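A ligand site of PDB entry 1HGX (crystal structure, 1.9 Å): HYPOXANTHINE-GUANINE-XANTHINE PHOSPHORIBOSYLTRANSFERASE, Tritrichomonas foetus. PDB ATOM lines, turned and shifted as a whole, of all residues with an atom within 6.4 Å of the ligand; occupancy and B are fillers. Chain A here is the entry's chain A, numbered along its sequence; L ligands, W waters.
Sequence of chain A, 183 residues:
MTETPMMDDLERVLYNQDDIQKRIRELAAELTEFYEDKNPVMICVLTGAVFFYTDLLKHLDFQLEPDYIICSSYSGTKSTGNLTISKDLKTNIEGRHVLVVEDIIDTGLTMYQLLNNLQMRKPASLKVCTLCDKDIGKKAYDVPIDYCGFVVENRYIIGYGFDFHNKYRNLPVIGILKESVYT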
ATOM      1  N   VAL A  45       5.137  36.400 -30.056  1.00  0.00           N
ATOM      2  CA  VAL A  45       5.039  36.305 -28.608  1.00  0.00           C
ATOM      3  C   VAL A  45       6.183  35.371 -28.179  1.00  0.00           C
ATOM      4  O   VAL A  45       6.118  34.151 -28.369  1.00  0.00           O
ATOM      5  CB  VAL A  45       3.663  35.770 -28.151  1.00  0.00           C
ATOM      6  CG1 VAL A  45       3.595  35.717 -26.622  1.00  0.00           C
ATOM      7  CG2 VAL A  45       2.522  36.653 -28.727  1.00  0.00           C
ATOM      8  N   GLY A  48       8.501  30.758 -26.941  1.00  0.00           N
ATOM      9  CA  GLY A  48       7.988  29.599 -27.661  1.00  0.00           C
ATOM     10  C   GLY A  48       7.628  29.714 -29.132  1.00  0.00           C
ATOM     11  O   GLY A  48       7.932  28.822 -29.919  1.00  0.00           O
ATOM     12  N   CYS A  71       5.015  38.579 -22.376  1.00  0.00           N
ATOM     13  CA  CYS A  71       3.953  38.766 -21.404  1.00  0.00           C
ATOM     14  C   CYS A  71       3.543  37.438 -20.788  1.00  0.00           C
ATOM     15  O   CYS A  71       4.014  36.394 -21.213  1.00  0.00           O
ATOM     16  CB  CYS A  71       2.750  39.409 -22.090  1.00  0.00           C
ATOM     17  SG  CYS A  71       2.140  38.463 -23.479  1.00  0.00           S
ATOM     18  N   SER A  73       0.006  35.589 -18.317  1.00  0.00           N
ATOM     19  CA  SER A  73      -1.236  35.764 -17.596  1.00  0.00           C
ATOM     20  C   SER A  73      -1.244  34.961 -16.289  1.00  0.00           C
ATOM     21  O   SER A  73      -0.344  34.162 -16.035  1.00  0.00           O
ATOM     22  CB  SER A  73      -2.411  35.336 -18.483  1.00  0.00           C
ATOM     23  OG  SER A  73      -2.487  36.171 -19.627  1.00  0.00           O
ATOM     24  N   GLU A 102       1.486  33.271 -32.159  1.00  0.00           N
ATOM     25  CA  GLU A 102       1.586  32.573 -30.885  1.00  0.00           C
ATOM     26  C   GLU A 102       1.938  31.086 -31.073  1.00  0.00           C
ATOM     27  O   GLU A 102       1.803  30.544 -32.171  1.00  0.00           O
ATOM     28  CB  GLU A 102       0.238  32.725 -30.142  1.00  0.00           C
ATOM     29  CG  GLU A 102       0.120  32.003 -28.800  1.00  0.00           C
ATOM     30  CD  GLU A 102       1.080  32.510 -27.730  1.00  0.00           C
ATOM     31  OE1 GLU A 102       2.308  32.362 -27.882  1.00  0.00           O
ATOM     32  OE2 GLU A 102       0.595  33.046 -26.717  1.00  0.00           O
ATOM     33  N   ASP A 103       2.436  30.466 -30.003  1.00  0.00           N
ATOM     34  CA  ASP A 103       2.801  29.057 -30.051  1.00  0.00           C
ATOM     35  C   ASP A 103       1.624  28.086 -29.815  1.00  0.00           C
ATOM     36  O   ASP A 103       1.363  27.220 -30.648  1.00  0.00           O
ATOM     37  CB  ASP A 103       4.014  28.726 -29.143  1.00  0.00           C
ATOM     38  CG  ASP A 103       3.873  29.238 -27.689  1.00  0.00           C
ATOM     39  OD1 ASP A 103       2.777  29.635 -27.230  1.00  0.00           O
ATOM     40  OD2 ASP A 103       4.902  29.227 -26.980  1.00  0.00           O
ATOM     41  N   ILE A 104       0.899  28.263 -28.714  1.00  0.00           N
ATOM     42  CA  ILE A 104      -0.225  27.389 -28.412  1.00  0.00           C
ATOM     43  C   ILE A 104      -1.254  28.115 -27.551  1.00  0.00           C
ATOM     44  O   ILE A 104      -0.912  28.953 -26.715  1.00  0.00           O
ATOM     45  CB  ILE A 104       0.248  26.089 -27.697  1.00  0.00           C
ATOM     46  CG1 ILE A 104      -0.922  25.110 -27.511  1.00  0.00           C
ATOM     47  CG2 ILE A 104       0.881  26.408 -26.356  1.00  0.00           C
ATOM     48  CD1 ILE A 104      -0.471  23.747 -27.058  1.00  0.00           C
ATOM     49  N   ILE A 105      -2.522  27.860 -27.841  1.00  0.00           N
ATOM     50  CA  ILE A 105      -3.624  28.446 -27.090  1.00  0.00           C
ATOM     51  C   ILE A 105      -4.267  27.307 -26.297  1.00  0.00           C
ATOM     52  O   ILE A 105      -4.709  26.302 -26.869  1.00  0.00           O
ATOM     53  CB  ILE A 105      -4.638  29.119 -28.035  1.00  0.00           C
ATOM     54  CG1 ILE A 105      -3.989  30.355 -28.665  1.00  0.00           C
ATOM     55  CG2 ILE A 105      -5.917  29.502 -27.266  1.00  0.00           C
ATOM     56  CD1 ILE A 105      -4.861  31.098 -29.629  1.00  0.00           C
ATOM     57  N   ASP A 106      -4.212  27.437 -24.974  1.00  0.00           N
ATOM     58  CA  ASP A 106      -4.752  26.446 -24.064  1.00  0.00           C
ATOM     59  C   ASP A 106      -6.159  26.852 -23.624  1.00  0.00           C
ATOM     60  O   ASP A 106      -7.131  26.565 -24.316  1.00  0.00           O
ATOM     61  CB  ASP A 106      -3.799  26.281 -22.876  1.00  0.00           C
ATOM     62  CG  ASP A 106      -4.137  25.094 -21.993  1.00  0.00           C
ATOM     63  OD1 ASP A 106      -5.217  24.489 -22.137  1.00  0.00           O
ATOM     64  OD2 ASP A 106      -3.289  24.776 -21.133  1.00  0.00           O
ATOM     65  N   THR A 107      -6.285  27.553 -22.492  1.00  0.00           N
ATOM     66  CA  THR A 107      -7.603  27.969 -22.029  1.00  0.00           C
ATOM     67  C   THR A 107      -8.061  29.236 -22.737  1.00  0.00           C
ATOM     68  O   THR A 107      -9.239  29.606 -22.662  1.00  0.00           O
ATOM     69  CB  THR A 107      -7.605  28.263 -20.522  1.00  0.00           C
ATOM     70  OG1 THR A 107      -6.803  29.424 -20.265  1.00  0.00           O
ATOM     71  CG2 THR A 107      -7.057  27.076 -19.741  1.00  0.00           C
ATOM     72  N   GLY A 108      -7.124  29.914 -23.385  1.00  0.00           N
ATOM     73  CA  GLY A 108      -7.467  31.129 -24.104  1.00  0.00           C
ATOM     74  C   GLY A 108      -7.274  32.407 -23.282  1.00  0.00           C
ATOM     75  O   GLY A 108      -7.393  33.501 -23.827  1.00  0.00           O
ATOM     76  N   LEU A 109      -6.959  32.271 -21.995  1.00  0.00           N
ATOM     77  CA  LEU A 109      -6.780  33.446 -21.135  1.00  0.00           C
ATOM     78  C   LEU A 109      -5.706  34.417 -21.628  1.00  0.00           C
ATOM     79  O   LEU A 109      -5.961  35.625 -21.744  1.00  0.00           O
ATOM     80  CB  LEU A 109      -6.462  33.013 -19.703  1.00  0.00           C
ATOM     81  CG  LEU A 109      -6.128  34.116 -18.698  1.00  0.00           C
ATOM     82  CD1 LEU A 109      -7.307  35.034 -18.479  1.00  0.00           C
ATOM     83  CD2 LEU A 109      -5.692  33.495 -17.388  1.00  0.00           C
ATOM     84  N   THR A 110      -4.501  33.926 -21.880  1.00  0.00           N
ATOM     85  CA  THR A 110      -3.409  34.761 -22.345  1.00  0.00           C
ATOM     86  C   THR A 110      -3.749  35.563 -23.600  1.00  0.00           C
ATOM     87  O   THR A 110      -3.632  36.798 -23.615  1.00  0.00           O
ATOM     88  CB  THR A 110      -2.124  33.939 -22.594  1.00  0.00           C
ATOM     89  OG1 THR A 110      -1.805  33.179 -21.419  1.00  0.00           O
ATOM     90  CG2 THR A 110      -0.954  34.871 -22.884  1.00  0.00           C
ATOM     91  N   MET A 111      -4.215  34.888 -24.642  1.00  0.00           N
ATOM     92  CA  MET A 111      -4.564  35.546 -25.884  1.00  0.00           C
ATOM     93  C   MET A 111      -5.762  36.489 -25.727  1.00  0.00           C
ATOM     94  O   MET A 111      -5.796  37.563 -26.339  1.00  0.00           O
ATOM     95  CB  MET A 111      -4.835  34.512 -26.988  1.00  0.00           C
ATOM     96  CG  MET A 111      -4.891  35.078 -28.397  1.00  0.00           C
ATOM     97  SD  MET A 111      -3.450  36.094 -28.831  1.00  0.00           S
ATOM     98  CE  MET A 111      -2.109  35.041 -28.394  1.00  0.00           C
ATOM     99  N   LYS A 134      -4.717  23.727 -28.379  1.00  0.00           N
ATOM    100  CA  LYS A 134      -4.943  22.564 -27.539  1.00  0.00           C
ATOM    101  C   LYS A 134      -6.442  22.300 -27.412  1.00  0.00           C
ATOM    102  O   LYS A 134      -7.203  23.179 -27.028  1.00  0.00           O
ATOM    103  CB  LYS A 134      -4.316  22.769 -26.154  1.00  0.00           C
ATOM    104  CG  LYS A 134      -4.331  21.506 -25.309  1.00  0.00           C
ATOM    105  CD  LYS A 134      -3.639  21.693 -23.964  1.00  0.00           C
ATOM    106  CE  LYS A 134      -2.165  21.931 -24.122  1.00  0.00           C
ATOM    107  NZ  LYS A 134      -1.447  21.815 -22.823  1.00  0.00           N
ATOM    108  N   VAL A 152      -4.034  20.149 -31.243  1.00  0.00           N
ATOM    109  CA  VAL A 152      -3.293  19.215 -30.419  1.00  0.00           C
ATOM    110  C   VAL A 152      -4.156  18.648 -29.277  1.00  0.00           C
ATOM    111  O   VAL A 152      -5.108  19.282 -28.850  1.00  0.00           O
ATOM    112  CB  VAL A 152      -2.023  19.939 -29.930  1.00  0.00           C
ATOM    113  CG1 VAL A 152      -2.085  20.267 -28.455  1.00  0.00           C
ATOM    114  CG2 VAL A 152      -0.787  19.187 -30.323  1.00  0.00           C
ATOM    115  N   ARG A 155      -2.542  17.399 -23.676  1.00  0.00           N
ATOM    116  CA  ARG A 155      -1.373  16.852 -22.984  1.00  0.00           C
ATOM    117  C   ARG A 155      -0.316  17.963 -22.989  1.00  0.00           C
ATOM    118  O   ARG A 155      -0.507  18.989 -23.651  1.00  0.00           O
ATOM    119  CB  ARG A 155      -0.818  15.620 -23.711  1.00  0.00           C
ATOM    120  CG  ARG A 155      -1.770  14.425 -23.853  1.00  0.00           C
ATOM    121  CD  ARG A 155      -2.068  13.749 -22.528  1.00  0.00           C
ATOM    122  NE  ARG A 155      -0.847  13.323 -21.859  1.00  0.00           N
ATOM    123  CZ  ARG A 155      -0.173  12.202 -22.124  1.00  0.00           C
ATOM    124  NH1 ARG A 155      -0.606  11.369 -23.068  1.00  0.00           N
ATOM    125  NH2 ARG A 155       0.951  11.949 -21.488  1.00  0.00           N
ATOM    126  N   TYR A 156       0.769  17.777 -22.247  1.00  0.00           N
ATOM    127  CA  TYR A 156       1.813  18.784 -22.213  1.00  0.00           C
ATOM    128  C   TYR A 156       2.670  18.618 -23.447  1.00  0.00           C
ATOM    129  O   TYR A 156       3.358  17.609 -23.596  1.00  0.00           O
ATOM    130  CB  TYR A 156       2.698  18.690 -20.962  1.00  0.00           C
ATOM    131  CG  TYR A 156       3.544  19.924 -20.778  1.00  0.00           C
ATOM    132  CD1 TYR A 156       3.011  21.089 -20.230  1.00  0.00           C
ATOM    133  CD2 TYR A 156       4.874  19.965 -21.224  1.00  0.00           C
ATOM    134  CE1 TYR A 156       3.752  22.241 -20.134  1.00  0.00           C
ATOM    135  CE2 TYR A 156       5.626  21.125 -21.129  1.00  0.00           C
ATOM    136  CZ  TYR A 156       5.056  22.256 -20.578  1.00  0.00           C
ATOM    137  OH  TYR A 156       5.794  23.412 -20.473  1.00  0.00           O
ATOM    138  N   ILE A 157       2.585  19.596 -24.338  1.00  0.00           N
ATOM    139  CA  ILE A 157       3.307  19.595 -25.591  1.00  0.00           C
ATOM    140  C   ILE A 157       4.749  20.069 -25.429  1.00  0.00           C
ATOM    141  O   ILE A 157       5.035  21.073 -24.746  1.00  0.00           O
ATOM    142  CB  ILE A 157       2.534  20.442 -26.658  1.00  0.00           C
ATOM    143  CG1 ILE A 157       1.111  19.892 -26.805  1.00  0.00           C
ATOM    144  CG2 ILE A 157       3.259  20.438 -28.010  1.00  0.00           C
ATOM    145  CD1 ILE A 157       1.032  18.365 -27.051  1.00  0.00           C
ATOM    146  N   ILE A 158       5.638  19.379 -26.122  1.00  0.00           N
ATOM    147  CA  ILE A 158       7.061  19.662 -26.056  1.00  0.00           C
ATOM    148  C   ILE A 158       7.689  19.636 -27.473  1.00  0.00           C
ATOM    149  O   ILE A 158       7.130  19.016 -28.386  1.00  0.00           O
ATOM    150  CB  ILE A 158       7.718  18.614 -25.086  1.00  0.00           C
ATOM    151  CG1 ILE A 158       8.697  19.304 -24.165  1.00  0.00           C
ATOM    152  CG2 ILE A 158       8.299  17.407 -25.816  1.00  0.00           C
ATOM    153  CD1 ILE A 158       8.039  20.312 -23.276  1.00  0.00           C
ATOM    154  N   GLY A 161      10.365  24.659 -30.157  1.00  0.00           N
ATOM    155  CA  GLY A 161      10.071  25.889 -29.451  1.00  0.00           C
ATOM    156  C   GLY A 161       9.400  25.673 -28.105  1.00  0.00           C
ATOM    157  O   GLY A 161       9.569  26.497 -27.203  1.00  0.00           O
ATOM    158  N   PHE A 162       8.602  24.612 -27.974  1.00  0.00           N
ATOM    159  CA  PHE A 162       7.916  24.307 -26.707  1.00  0.00           C
ATOM    160  C   PHE A 162       8.917  23.677 -25.740  1.00  0.00           C
ATOM    161  O   PHE A 162       9.536  22.656 -26.063  1.00  0.00           O
ATOM    162  CB  PHE A 162       6.775  23.303 -26.918  1.00  0.00           C
ATOM    163  CG  PHE A 162       5.637  23.844 -27.734  1.00  0.00           C
ATOM    164  CD1 PHE A 162       4.828  24.849 -27.236  1.00  0.00           C
ATOM    165  CD2 PHE A 162       5.370  23.329 -28.995  1.00  0.00           C
ATOM    166  CE1 PHE A 162       3.756  25.345 -27.980  1.00  0.00           C
ATOM    167  CE2 PHE A 162       4.299  23.812 -29.743  1.00  0.00           C
ATOM    168  CZ  PHE A 162       3.487  24.821 -29.237  1.00  0.00           C
ATOM    169  N   ASP A 163       9.062  24.277 -24.562  1.00  0.00           N
ATOM    170  CA  ASP A 163      10.001  23.770 -23.562  1.00  0.00           C
ATOM    171  C   ASP A 163       9.309  23.316 -22.292  1.00  0.00           C
ATOM    172  O   ASP A 163       8.121  23.588 -22.067  1.00  0.00           O
ATOM    173  CB  ASP A 163      11.003  24.870 -23.163  1.00  0.00           C
ATOM    174  CG  ASP A 163      10.409  25.860 -22.157  1.00  0.00           C
ATOM    175  OD1 ASP A 163       9.639  26.746 -22.577  1.00  0.00           O
ATOM    176  OD2 ASP A 163      10.699  25.747 -20.944  1.00  0.00           O
ATOM    177  N   PHE A 164      10.079  22.656 -21.437  1.00  0.00           N
ATOM    178  CA  PHE A 164       9.650  22.224 -20.119  1.00  0.00           C
ATOM    179  C   PHE A 164      10.902  22.435 -19.277  1.00  0.00           C
ATOM    180  O   PHE A 164      11.921  21.778 -19.505  1.00  0.00           O
ATOM    181  CB  PHE A 164       9.256  20.745 -20.087  1.00  0.00           C
ATOM    182  CG  PHE A 164       8.982  20.239 -18.690  1.00  0.00           C
ATOM    183  CD1 PHE A 164       7.830  20.628 -18.009  1.00  0.00           C
ATOM    184  CD2 PHE A 164       9.902  19.434 -18.034  1.00  0.00           C
ATOM    185  CE1 PHE A 164       7.607  20.223 -16.695  1.00  0.00           C
ATOM    186  CE2 PHE A 164       9.700  19.036 -16.717  1.00  0.00           C
ATOM    187  CZ  PHE A 164       8.550  19.422 -16.044  1.00  0.00           C
HETATM  188  P1  LIG L   1      -3.697  29.850 -21.906  1.00  0.00           P
HETATM  189  O1  LIG L   1      -4.273  29.719 -23.262  1.00  0.00           O
HETATM  190  O2  LIG L   1      -3.684  31.224 -21.426  1.00  0.00           O
HETATM  191  O3  LIG L   1      -4.316  28.871 -20.980  1.00  0.00           O
HETATM  192  O4  LIG L   1      -2.255  29.280 -22.009  1.00  0.00           O
HETATM  193  C1  LIG L   1      -1.372  29.454 -23.118  1.00  0.00           C
HETATM  194  C2  LIG L   1      -0.020  29.711 -22.579  1.00  0.00           C
HETATM  195  O5  LIG L   1       0.527  28.587 -21.870  1.00  0.00           O
HETATM  196  C3  LIG L   1       0.948  30.045 -23.672  1.00  0.00           C
HETATM  197  O6  LIG L   1       1.943  30.848 -23.040  1.00  0.00           O
HETATM  198  C4  LIG L   1       1.505  28.698 -23.946  1.00  0.00           C
HETATM  199  O7  LIG L   1       2.788  28.818 -24.540  1.00  0.00           O
HETATM  200  C5  LIG L   1       1.598  27.983 -22.600  1.00  0.00           C
HETATM  201  N1  LIG L   1       1.280  26.510 -22.783  1.00  0.00           N
HETATM  202  C6  LIG L   1       0.021  25.949 -22.887  1.00  0.00           C
HETATM  203  N2  LIG L   1       0.018  24.656 -23.095  1.00  0.00           N
HETATM  204  C7  LIG L   1       1.374  24.304 -23.157  1.00  0.00           C
HETATM  205  C8  LIG L   1       1.962  23.048 -23.493  1.00  0.00           C
HETATM  206  O8  LIG L   1       1.402  21.960 -23.628  1.00  0.00           O
HETATM  207  N3  LIG L   1       3.342  23.125 -23.647  1.00  0.00           N
HETATM  208  C9  LIG L   1       4.078  24.294 -23.503  1.00  0.00           C
HETATM  209  N4  LIG L   1       5.410  24.184 -23.572  1.00  0.00           N
HETATM  210  N5  LIG L   1       3.530  25.482 -23.149  1.00  0.00           N
HETATM  211  C10 LIG L   1       2.163  25.435 -23.026  1.00  0.00           C
HETATM  212  O   HOH W   1       7.380  26.466 -24.156  1.00  0.00           O
HETATM  213  O   HOH W   2      -2.980  27.180 -19.101  1.00  0.00           O
HETATM  214  O   HOH W   3       2.479  33.152 -24.696  1.00  0.00           O
HETATM  215  O   HOH W   4      -4.350  32.053 -24.858  1.00  0.00           O
HETATM  216  O   HOH W   5       5.296  27.878 -24.763  1.00  0.00           O
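N of Thr 107 sits at hydrogen-bond distance from O3 of the ligand (2.8 Å). OG1 of Thr 107 sits at hydrogen-bond distance from O3 of the ligand (2.6 Å). An oxygen (O2) of the ligand is in hydrogen-bond range of the backbone NH (N) of Thr 110 (2.9 Å). An oxygen (O2) of the ligand lies within hydrogen-bond range of the side-chain hydroxyl (OG1) of Thr 110, at 2.7 Å. An oxygen (O8) of the ligand is in hydrogen-bond range of the backbone NH (N) of Ile 157. A nitrogen (N3) of the ligand lies within hydrogen-bond range of the backbone carbonyl oxygen (O) of Ile 157 (2.9 Å). The side-chain carboxylate (OD1) of Asp 103 lies within hydrogen-bond range of an oxygen (O7) of the ligand (2.8 Å). An oxygen (O1) of the ligand is in hydrogen-bond range of the backbone NH (N) of Asp 106, at 2.9 Å. The backbone NH (N) of Gly 108 sits at hydrogen-bond distance from an oxygen (O1) of the ligand (2.9 Å). The side-chain amino group (NZ) of Lys 134 sits at hydrogen-bond distance from an oxygen (O8) of the ligand. The backbone carbonyl oxygen (O) of Asp 163 lies within hydrogen-bond range of a nitrogen (N4) of the ligand (3.2 Å). N4 of the ligand lies within hydrogen-bond range of OH of Tyr 156, at 3.2 Å. N of Leu 109 is in hydrogen-bond range of O2 of the ligand (3.5 Å).
The backbone NH of Leu 109 lies close to the side-chain hydroxyl of Thr 107, at 3.3 Å. The side-chain carboxylate (OD2) of Asp 106 is in salt-bridge range of the side-chain amino group (NZ) of Lys 134, 3.9 Å away. The side-chain amino group of Lys 134 is in hydrogen-bond range of the backbone carbonyl oxygen of Arg 155 (3.1 Å). The backbone NH (N) of Lys 134 is in hydrogen-bond range of the backbone carbonyl oxygen (O) of Ile 105, at 3.0 Å. The backbone carbonyl oxygen (O) of Asp 163 is in hydrogen-bond range of the side-chain hydroxyl (OH) of Tyr 156 (2.8 Å).
Residues that only touch the ligand: Ile 104, Arg 155, Phe 162 and Ile 105. Along chain A the residues within 4 Å of the ligand span positions 103 to 163. The nearest printed residue that does not touch the ligand is Glu 102 (4.3 Å).
Water W5 lies within hydrogen-bond range of OD2 of Asp 103 (2.6 Å) and O7 of the ligand (2.7 Å). Water W4 lies within hydrogen-bond range of O1 of the ligand (2.8 Å) and N of Met 111 (2.8 Å). Water W2 bridges O3 of the ligand (2.9 Å) and OD2 of Asp 106 (3.2 Å). Water W3 bridges OE2 of Glu 102 (2.8 Å) and O6 of the ligand (2.9 Å). Water W1 lies within hydrogen-bond range of the side-chain carboxylate of Asp 163 (2.8 Å) and a nitrogen (N4) of the ligand (3.1 Å).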
